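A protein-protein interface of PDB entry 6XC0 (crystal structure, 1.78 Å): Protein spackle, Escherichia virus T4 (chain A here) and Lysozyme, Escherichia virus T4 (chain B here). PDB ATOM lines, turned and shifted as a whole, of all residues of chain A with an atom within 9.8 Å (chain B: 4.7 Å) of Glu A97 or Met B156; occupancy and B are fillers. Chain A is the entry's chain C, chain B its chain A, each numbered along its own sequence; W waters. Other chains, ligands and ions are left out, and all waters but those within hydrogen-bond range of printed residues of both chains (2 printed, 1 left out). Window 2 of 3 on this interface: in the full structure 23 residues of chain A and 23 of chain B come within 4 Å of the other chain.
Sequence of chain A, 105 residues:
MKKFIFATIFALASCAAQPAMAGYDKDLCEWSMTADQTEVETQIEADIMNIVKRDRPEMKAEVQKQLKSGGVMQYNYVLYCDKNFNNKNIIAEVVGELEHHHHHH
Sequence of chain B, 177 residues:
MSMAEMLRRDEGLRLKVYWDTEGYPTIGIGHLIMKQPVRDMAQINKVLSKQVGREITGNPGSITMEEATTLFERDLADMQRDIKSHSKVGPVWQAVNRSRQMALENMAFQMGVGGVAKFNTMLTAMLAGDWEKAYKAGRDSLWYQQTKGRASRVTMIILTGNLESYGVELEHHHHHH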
ATOM      1  N   ARG A  56      28.449  26.577  16.415  1.00  0.00           N
ATOM      2  CA  ARG A  56      27.875  26.395  15.077  1.00  0.00           C
ATOM      3  C   ARG A  56      26.405  26.777  15.108  1.00  0.00           C
ATOM      4  O   ARG A  56      25.521  25.920  14.968  1.00  0.00           O
ATOM      5  CB  ARG A  56      28.062  24.954  14.593  1.00  0.00           C
ATOM      6  CG  ARG A  56      29.473  24.675  14.104  1.00  0.00           C
ATOM      7  CD  ARG A  56      29.698  23.217  13.844  1.00  0.00           C
ATOM      8  NE  ARG A  56      28.956  22.775  12.665  1.00  0.00           N
ATOM      9  CZ  ARG A  56      28.840  21.503  12.279  1.00  0.00           C
ATOM     10  NH1 ARG A  56      28.141  21.225  11.183  1.00  0.00           N
ATOM     11  NH2 ARG A  56      29.432  20.515  12.967  1.00  0.00           N
ATOM     12  N   MET A  59      23.512  25.421  13.012  1.00  0.00           N
ATOM     13  CA  MET A  59      23.122  24.014  13.134  1.00  0.00           C
ATOM     14  C   MET A  59      21.991  23.791  14.151  1.00  0.00           C
ATOM     15  O   MET A  59      21.606  22.643  14.375  1.00  0.00           O
ATOM     16  CB  MET A  59      24.345  23.157  13.496  1.00  0.00           C
ATOM     17  CG  MET A  59      25.436  23.125  12.430  1.00  0.00           C
ATOM     18  SD  MET A  59      24.797  22.530  10.822  1.00  0.00           S
ATOM     19  CE  MET A  59      24.459  20.840  11.280  1.00  0.00           C
ATOM     20  N   ASN A  89      32.780  18.433  21.085  1.00  0.00           N
ATOM     21  CA  ASN A  89      32.484  17.537  19.970  1.00  0.00           C
ATOM     22  C   ASN A  89      31.061  16.981  20.009  1.00  0.00           C
ATOM     23  O   ASN A  89      30.734  16.077  19.229  1.00  0.00           O
ATOM     24  CB  ASN A  89      33.508  16.396  19.922  1.00  0.00           C
ATOM     25  CG  ASN A  89      34.907  16.885  19.626  1.00  0.00           C
ATOM     26  OD1 ASN A  89      35.105  17.797  18.818  1.00  0.00           O
ATOM     27  ND2 ASN A  89      35.899  16.325  20.328  1.00  0.00           N
ATOM     28  N   ILE A  90      30.208  17.486  20.903  1.00  0.00           N
ATOM     29  CA  ILE A  90      28.864  16.948  20.985  1.00  0.00           C
ATOM     30  C   ILE A  90      28.044  17.335  19.751  1.00  0.00           C
ATOM     31  O   ILE A  90      27.084  16.635  19.414  1.00  0.00           O
ATOM     32  CB  ILE A  90      28.159  17.406  22.280  1.00  0.00           C
ATOM     33  CG1 ILE A  90      26.969  16.500  22.569  1.00  0.00           C
ATOM     34  CG2 ILE A  90      27.741  18.928  22.148  1.00  0.00           C
ATOM     35  CD1 ILE A  90      27.401  15.069  23.017  1.00  0.00           C
ATOM     36  N   ILE A  91      28.395  18.424  19.057  1.00  0.00           N
ATOM     37  CA  ILE A  91      27.635  18.760  17.848  1.00  0.00           C
ATOM     38  C   ILE A  91      27.791  17.633  16.830  1.00  0.00           C
ATOM     39  O   ILE A  91      26.801  17.057  16.363  1.00  0.00           O
ATOM     40  CB  ILE A  91      28.061  20.120  17.259  1.00  0.00           C
ATOM     41  CG1 ILE A  91      28.041  21.233  18.345  1.00  0.00           C
ATOM     42  CG2 ILE A  91      27.074  20.512  16.167  1.00  0.00           C
ATOM     43  CD1 ILE A  91      28.349  22.631  17.785  1.00  0.00           C
ATOM     44  N   ALA A  92      29.048  17.247  16.544  1.00  0.00           N
ATOM     45  CA  ALA A  92      29.303  16.160  15.598  1.00  0.00           C
ATOM     46  C   ALA A  92      28.772  14.844  16.130  1.00  0.00           C
ATOM     47  O   ALA A  92      28.389  13.975  15.351  1.00  0.00           O
ATOM     48  CB  ALA A  92      30.798  16.040  15.290  1.00  0.00           C
ATOM     49  N   GLU A  93      28.717  14.683  17.448  1.00  0.00           N
ATOM     50  CA  GLU A  93      28.108  13.487  18.016  1.00  0.00           C
ATOM     51  C   GLU A  93      26.636  13.356  17.621  1.00  0.00           C
ATOM     52  O   GLU A  93      26.146  12.249  17.401  1.00  0.00           O
ATOM     53  CB  GLU A  93      28.210  13.505  19.542  1.00  0.00           C
ATOM     54  CG  GLU A  93      27.861  12.130  20.137  1.00  0.00           C
ATOM     55  CD  GLU A  93      29.032  11.133  19.998  1.00  0.00           C
ATOM     56  OE1 GLU A  93      30.113  11.536  19.474  1.00  0.00           O
ATOM     57  OE2 GLU A  93      28.872   9.945  20.398  1.00  0.00           O
ATOM     58  N   VAL A  94      25.916  14.472  17.559  1.00  0.00           N
ATOM     59  CA  VAL A  94      24.485  14.458  17.247  1.00  0.00           C
ATOM     60  C   VAL A  94      24.254  14.439  15.737  1.00  0.00           C
ATOM     61  O   VAL A  94      23.382  13.715  15.246  1.00  0.00           O
ATOM     62  CB  VAL A  94      23.793  15.687  17.876  1.00  0.00           C
ATOM     63  CG1 VAL A  94      22.343  15.807  17.377  1.00  0.00           C
ATOM     64  CG2 VAL A  94      23.779  15.577  19.382  1.00  0.00           C
ATOM     65  N   VAL A  95      24.996  15.245  14.983  1.00  0.00           N
ATOM     66  CA  VAL A  95      24.677  15.424  13.567  1.00  0.00           C
ATOM     67  C   VAL A  95      25.666  14.767  12.622  1.00  0.00           C
ATOM     68  O   VAL A  95      25.422  14.771  11.398  1.00  0.00           O
ATOM     69  CB  VAL A  95      24.517  16.915  13.193  1.00  0.00           C
ATOM     70  CG1 VAL A  95      23.511  17.585  14.139  1.00  0.00           C
ATOM     71  CG2 VAL A  95      25.867  17.647  13.178  1.00  0.00           C
ATOM     72  N   GLY A  96      26.750  14.201  13.126  1.00  0.00           N
ATOM     73  CA  GLY A  96      27.736  13.581  12.276  1.00  0.00           C
ATOM     74  C   GLY A  96      28.916  14.499  12.005  1.00  0.00           C
ATOM     75  O   GLY A  96      28.842  15.726  12.151  1.00  0.00           O
ATOM     76  N   GLU A  97      30.006  13.878  11.549  1.00  0.00           N
ATOM     77  CA  GLU A  97      31.285  14.555  11.382  1.00  0.00           C
ATOM     78  C   GLU A  97      31.173  15.752  10.444  1.00  0.00           C
ATOM     79  O   GLU A  97      30.368  15.769   9.506  1.00  0.00           O
ATOM     80  CB  GLU A  97      32.340  13.589  10.841  1.00  0.00           C
ATOM     81  CG  GLU A  97      32.339  13.459   9.317  1.00  0.00           C
ATOM     82  CD  GLU A  97      31.171  12.637   8.778  1.00  0.00           C
ATOM     83  OE1 GLU A  97      31.289  11.387   8.758  1.00  0.00           O
ATOM     84  OE2 GLU A  97      30.143  13.240   8.381  1.00  0.00           O
ATOM     85  N   LEU A  98      32.024  16.747  10.705  1.00  0.00           N
ATOM     86  CA  LEU A  98      32.055  18.007   9.971  1.00  0.00           C
ATOM     87  C   LEU A  98      30.734  18.710  10.247  1.00  0.00           C
ATOM     88  O   LEU A  98      30.047  18.387  11.219  1.00  0.00           O
ATOM     89  CB  LEU A  98      32.286  17.791   8.464  1.00  0.00           C
ATOM     90  CG  LEU A  98      33.322  16.753   8.008  1.00  0.00           C
ATOM     91  CD1 LEU A  98      33.228  16.535   6.504  1.00  0.00           C
ATOM     92  CD2 LEU A  98      34.737  17.158   8.401  1.00  0.00           C
ATOM     93  N   TYR B 135      28.986   2.359   2.146  1.00  0.00           N
ATOM     94  CA  TYR B 135      28.906   3.601   2.914  1.00  0.00           C
ATOM     95  C   TYR B 135      27.818   4.539   2.392  1.00  0.00           C
ATOM     96  O   TYR B 135      27.020   5.090   3.169  1.00  0.00           O
ATOM     97  CB  TYR B 135      30.284   4.261   2.842  1.00  0.00           C
ATOM     98  CG  TYR B 135      30.406   5.699   3.298  1.00  0.00           C
ATOM     99  CD1 TYR B 135      30.596   5.992   4.634  1.00  0.00           C
ATOM    100  CD2 TYR B 135      30.459   6.744   2.377  1.00  0.00           C
ATOM    101  CE1 TYR B 135      30.769   7.298   5.063  1.00  0.00           C
ATOM    102  CE2 TYR B 135      30.635   8.067   2.797  1.00  0.00           C
ATOM    103  CZ  TYR B 135      30.793   8.320   4.155  1.00  0.00           C
ATOM    104  OH  TYR B 135      30.959   9.592   4.645  1.00  0.00           O
ATOM    105  N   ARG B 139      24.352   5.736   4.220  1.00  0.00           N
ATOM    106  CA  ARG B 139      24.046   7.148   4.443  1.00  0.00           C
ATOM    107  C   ARG B 139      22.841   7.637   3.659  1.00  0.00           C
ATOM    108  O   ARG B 139      22.301   8.707   3.985  1.00  0.00           O
ATOM    109  CB  ARG B 139      25.280   8.019   4.142  1.00  0.00           C
ATOM    110  CG  ARG B 139      26.430   7.749   5.097  1.00  0.00           C
ATOM    111  CD  ARG B 139      27.312   8.970   5.333  1.00  0.00           C
ATOM    112  NE  ARG B 139      28.233   8.726   6.443  1.00  0.00           N
ATOM    113  CZ  ARG B 139      29.022   9.658   6.944  1.00  0.00           C
ATOM    114  NH1 ARG B 139      28.976  10.894   6.441  1.00  0.00           N
ATOM    115  NH2 ARG B 139      29.846   9.353   7.927  1.00  0.00           N
ATOM    116  N   ALA B 151      24.530   7.000  12.843  1.00  0.00           N
ATOM    117  CA  ALA B 151      24.703   6.415  11.511  1.00  0.00           C
ATOM    118  C   ALA B 151      26.014   6.871  10.856  1.00  0.00           C
ATOM    119  O   ALA B 151      26.658   6.108  10.111  1.00  0.00           O
ATOM    120  CB  ALA B 151      23.512   6.787  10.626  1.00  0.00           C
ATOM    121  N   SER B 152      26.387   8.141  11.057  1.00  0.00           N
ATOM    122  CA  SER B 152      27.664   8.631  10.553  1.00  0.00           C
ATOM    123  C   SER B 152      28.837   7.823  11.094  1.00  0.00           C
ATOM    124  O   SER B 152      29.703   7.380  10.330  1.00  0.00           O
ATOM    125  CB  SER B 152      27.853  10.098  10.928  1.00  0.00           C
ATOM    126  OG  SER B 152      29.027  10.561  10.320  1.00  0.00           O
ATOM    127  N   ARG B 153      28.925   7.691  12.426  1.00  0.00           N
ATOM    128  CA  ARG B 153      30.037   6.942  13.030  1.00  0.00           C
ATOM    129  C   ARG B 153      30.058   5.514  12.539  1.00  0.00           C
ATOM    130  O   ARG B 153      31.139   4.952  12.314  1.00  0.00           O
ATOM    131  CB  ARG B 153      29.932   6.901  14.566  1.00  0.00           C
ATOM    132  CG  ARG B 153      30.049   8.248  15.220  1.00  0.00           C
ATOM    133  CD  ARG B 153      30.068   8.099  16.785  1.00  0.00           C
ATOM    134  NE  ARG B 153      28.768   7.807  17.422  1.00  0.00           N
ATOM    135  CZ  ARG B 153      27.792   8.716  17.560  1.00  0.00           C
ATOM    136  NH1 ARG B 153      27.935   9.935  17.062  1.00  0.00           N
ATOM    137  NH2 ARG B 153      26.663   8.412  18.162  1.00  0.00           N
ATOM    138  N   VAL B 154      28.877   4.896  12.427  1.00  0.00           N
ATOM    139  CA  VAL B 154      28.811   3.472  12.084  1.00  0.00           C
ATOM    140  C   VAL B 154      29.173   3.259  10.619  1.00  0.00           C
ATOM    141  O   VAL B 154      29.970   2.368  10.289  1.00  0.00           O
ATOM    142  CB  VAL B 154      27.429   2.902  12.430  1.00  0.00           C
ATOM    143  CG1 VAL B 154      27.181   1.542  11.758  1.00  0.00           C
ATOM    144  CG2 VAL B 154      27.255   2.798  14.001  1.00  0.00           C
ATOM    145  N   THR B 155      28.614   4.081   9.726  1.00  0.00           N
ATOM    146  CA  THR B 155      28.971   3.936   8.299  1.00  0.00           C
ATOM    147  C   THR B 155      30.435   4.289   8.035  1.00  0.00           C
ATOM    148  O   THR B 155      31.029   3.796   7.068  1.00  0.00           O
ATOM    149  CB  THR B 155      28.072   4.792   7.409  1.00  0.00           C
ATOM    150  OG1 THR B 155      28.148   6.157   7.829  1.00  0.00           O
ATOM    151  CG2 THR B 155      26.608   4.293   7.447  1.00  0.00           C
ATOM    152  N   MET B 156      31.036   5.158   8.845  1.00  0.00           N
ATOM    153  CA  MET B 156      32.455   5.441   8.673  1.00  0.00           C
ATOM    154  C   MET B 156      33.283   4.190   8.920  1.00  0.00           C
ATOM    155  O   MET B 156      34.304   3.973   8.249  1.00  0.00           O
ATOM    156  CB  MET B 156      32.898   6.574   9.603  1.00  0.00           C
ATOM    157  CG  MET B 156      34.279   7.185   9.309  1.00  0.00           C
ATOM    158  SD  MET B 156      34.378   7.886   7.576  1.00  0.00           S
ATOM    159  CE  MET B 156      32.992   8.962   7.563  1.00  0.00           C
ATOM    160  N   ILE B 157      32.851   3.344   9.868  1.00  0.00           N
ATOM    161  CA  ILE B 157      33.541   2.061  10.062  1.00  0.00           C
ATOM    162  C   ILE B 157      33.457   1.218   8.801  1.00  0.00           C
ATOM    163  O   ILE B 157      34.435   0.576   8.384  1.00  0.00           O
ATOM    164  CB  ILE B 157      32.950   1.285  11.242  1.00  0.00           C
ATOM    165  CG1 ILE B 157      33.158   2.038  12.544  1.00  0.00           C
ATOM    166  CG2 ILE B 157      33.612  -0.115  11.289  1.00  0.00           C
ATOM    167  CD1 ILE B 157      32.337   1.361  13.677  1.00  0.00           C
ATOM    168  N   ILE B 158      32.261   1.138   8.230  1.00  0.00           N
ATOM    169  CA  ILE B 158      32.060   0.314   7.050  1.00  0.00           C
ATOM    170  C   ILE B 158      32.959   0.788   5.918  1.00  0.00           C
ATOM    171  O   ILE B 158      33.503  -0.014   5.155  1.00  0.00           O
ATOM    172  CB  ILE B 158      30.574   0.333   6.658  1.00  0.00           C
ATOM    173  CG1 ILE B 158      29.763  -0.459   7.702  1.00  0.00           C
ATOM    174  CG2 ILE B 158      30.401  -0.256   5.257  1.00  0.00           C
ATOM    175  CD1 ILE B 158      28.273  -0.256   7.540  1.00  0.00           C
ATOM    176  N   LEU B 159      33.122   2.107   5.786  1.00  0.00           N
ATOM    177  CA  LEU B 159      33.980   2.652   4.747  1.00  0.00           C
ATOM    178  C   LEU B 159      35.458   2.337   5.001  1.00  0.00           C
ATOM    179  O   LEU B 159      36.173   1.924   4.085  1.00  0.00           O
ATOM    180  CB  LEU B 159      33.812   4.167   4.687  1.00  0.00           C
ATOM    181  CG  LEU B 159      34.699   4.880   3.648  1.00  0.00           C
ATOM    182  CD1 LEU B 159      34.252   4.391   2.262  1.00  0.00           C
ATOM    183  CD2 LEU B 159      34.510   6.392   3.740  1.00  0.00           C
ATOM    184  N   THR B 160      35.960   2.614   6.218  1.00  0.00           N
ATOM    185  CA  THR B 160      37.404   2.616   6.470  1.00  0.00           C
ATOM    186  C   THR B 160      37.924   1.286   6.993  1.00  0.00           C
ATOM    187  O   THR B 160      39.126   0.990   6.865  1.00  0.00           O
ATOM    188  CB  THR B 160      37.795   3.673   7.508  1.00  0.00           C
ATOM    189  OG1 THR B 160      37.172   3.316   8.749  1.00  0.00           O
ATOM    190  CG2 THR B 160      37.377   5.060   7.085  1.00  0.00           C
ATOM    191  N   GLY B 161      37.046   0.500   7.579  1.00  0.00           N
ATOM    192  CA  GLY B 161      37.438  -0.753   8.130  1.00  0.00           C
ATOM    193  C   GLY B 161      38.105  -0.642   9.472  1.00  0.00           C
ATOM    194  O   GLY B 161      38.676  -1.638   9.934  1.00  0.00           O
ATOM    195  N   SER B 165      36.395   6.407  13.950  1.00  0.00           N
ATOM    196  CA  SER B 165      35.232   7.263  14.168  1.00  0.00           C
ATOM    197  C   SER B 165      34.718   7.182  15.594  1.00  0.00           C
ATOM    198  O   SER B 165      33.894   8.017  15.972  1.00  0.00           O
ATOM    199  CB  SER B 165      34.089   6.931  13.190  1.00  0.00           C
ATOM    200  OG  SER B 165      33.564   5.622  13.348  1.00  0.00           O
HETATM  201  O   HOH W   1      29.881  11.489  15.354  1.00  0.00           O
HETATM  202  O   HOH W   2      30.653  11.242  12.615  1.00  0.00           O
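Printed residues of chain A that touch a printed residue of chain B: Glu A93, Gly A96 and Glu A97. Of the 14 printed residues of chain B, 4 touch a printed residue of chain A. Among the printed residues, 5 pairs touch across the chains. Among the printed residues, Asp or Glu carboxylates within 4 Å of a Lys or Arg side-chain nitrogen of the other chain: Glu A93 with Arg B153 (3.5 Å) and Glu A97 with Arg B139 (2.6 Å).
Arg A56 touches none of the printed residues of chain B. Of the printed residues of chain B, Glu A93 touches Arg B153. Printed residues of chain B within 4 Å of Gly A96: Ser B152. Printed residues of chain B within 4 Å of Glu A97: Arg B139 (2.6 Å), Ser B152 (2.9 Å) and Met B156 (3.2 Å). No residue of chain A comes within 4 Å of Thr B155. Met B156 touches one residue of chain A. Gly B161 touches none of the printed residues of chain A. The nearest printed residue of chain B that does not touch Glu A97 is Tyr B135 (4.5 Å). The nearest residue of chain A that does not touch Met B156 is Leu A98 (7.7 Å).
Among the printed residues, merely in contact across the chains: Glu A97 with Met B156 and Gly A96 with Ser B152.
The guanidinium group of Arg B139 sits at hydrogen-bond distance from the side-chain hydroxyl of Tyr B135 (3.0 Å). NH2 of Arg B139 is in hydrogen-bond range of OG of Ser B152. The guanidinium group (NE) of Arg B139 is in hydrogen-bond range of the side-chain hydroxyl (OG1) of Thr B155. OG1 of Thr B155 sits at hydrogen-bond distance from O of Ser B152, 3.2 Å away. O of Arg B153 lies within hydrogen-bond range of OG of Ser B165, at 2.7 Å. O of Met B156 lies within hydrogen-bond range of OG1 of Thr B160 (3.0 Å).
The guanidinium group (NH2) of Arg B139 lies within salt-bridge range of the side-chain carboxylate (OE1) of Glu A97. The side-chain hydroxyl of Ser B152 sits at hydrogen-bond distance from the side-chain carboxylate of Glu A97. The guanidinium group (NH1) of Arg B153 lies within salt-bridge range of the side-chain carboxylate (OE2) of Glu A93, 3.5 Å away.
Water W2 lies within hydrogen-bond range of OG of Ser B152 (2.9 Å) and N of Glu A97 (2.9 Å). Water W1 lies within hydrogen-bond range of the backbone carbonyl oxygen (O) of Ala A92 (2.9 Å) and the guanidinium group (NH1) of Arg B153 (3.0 Å).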
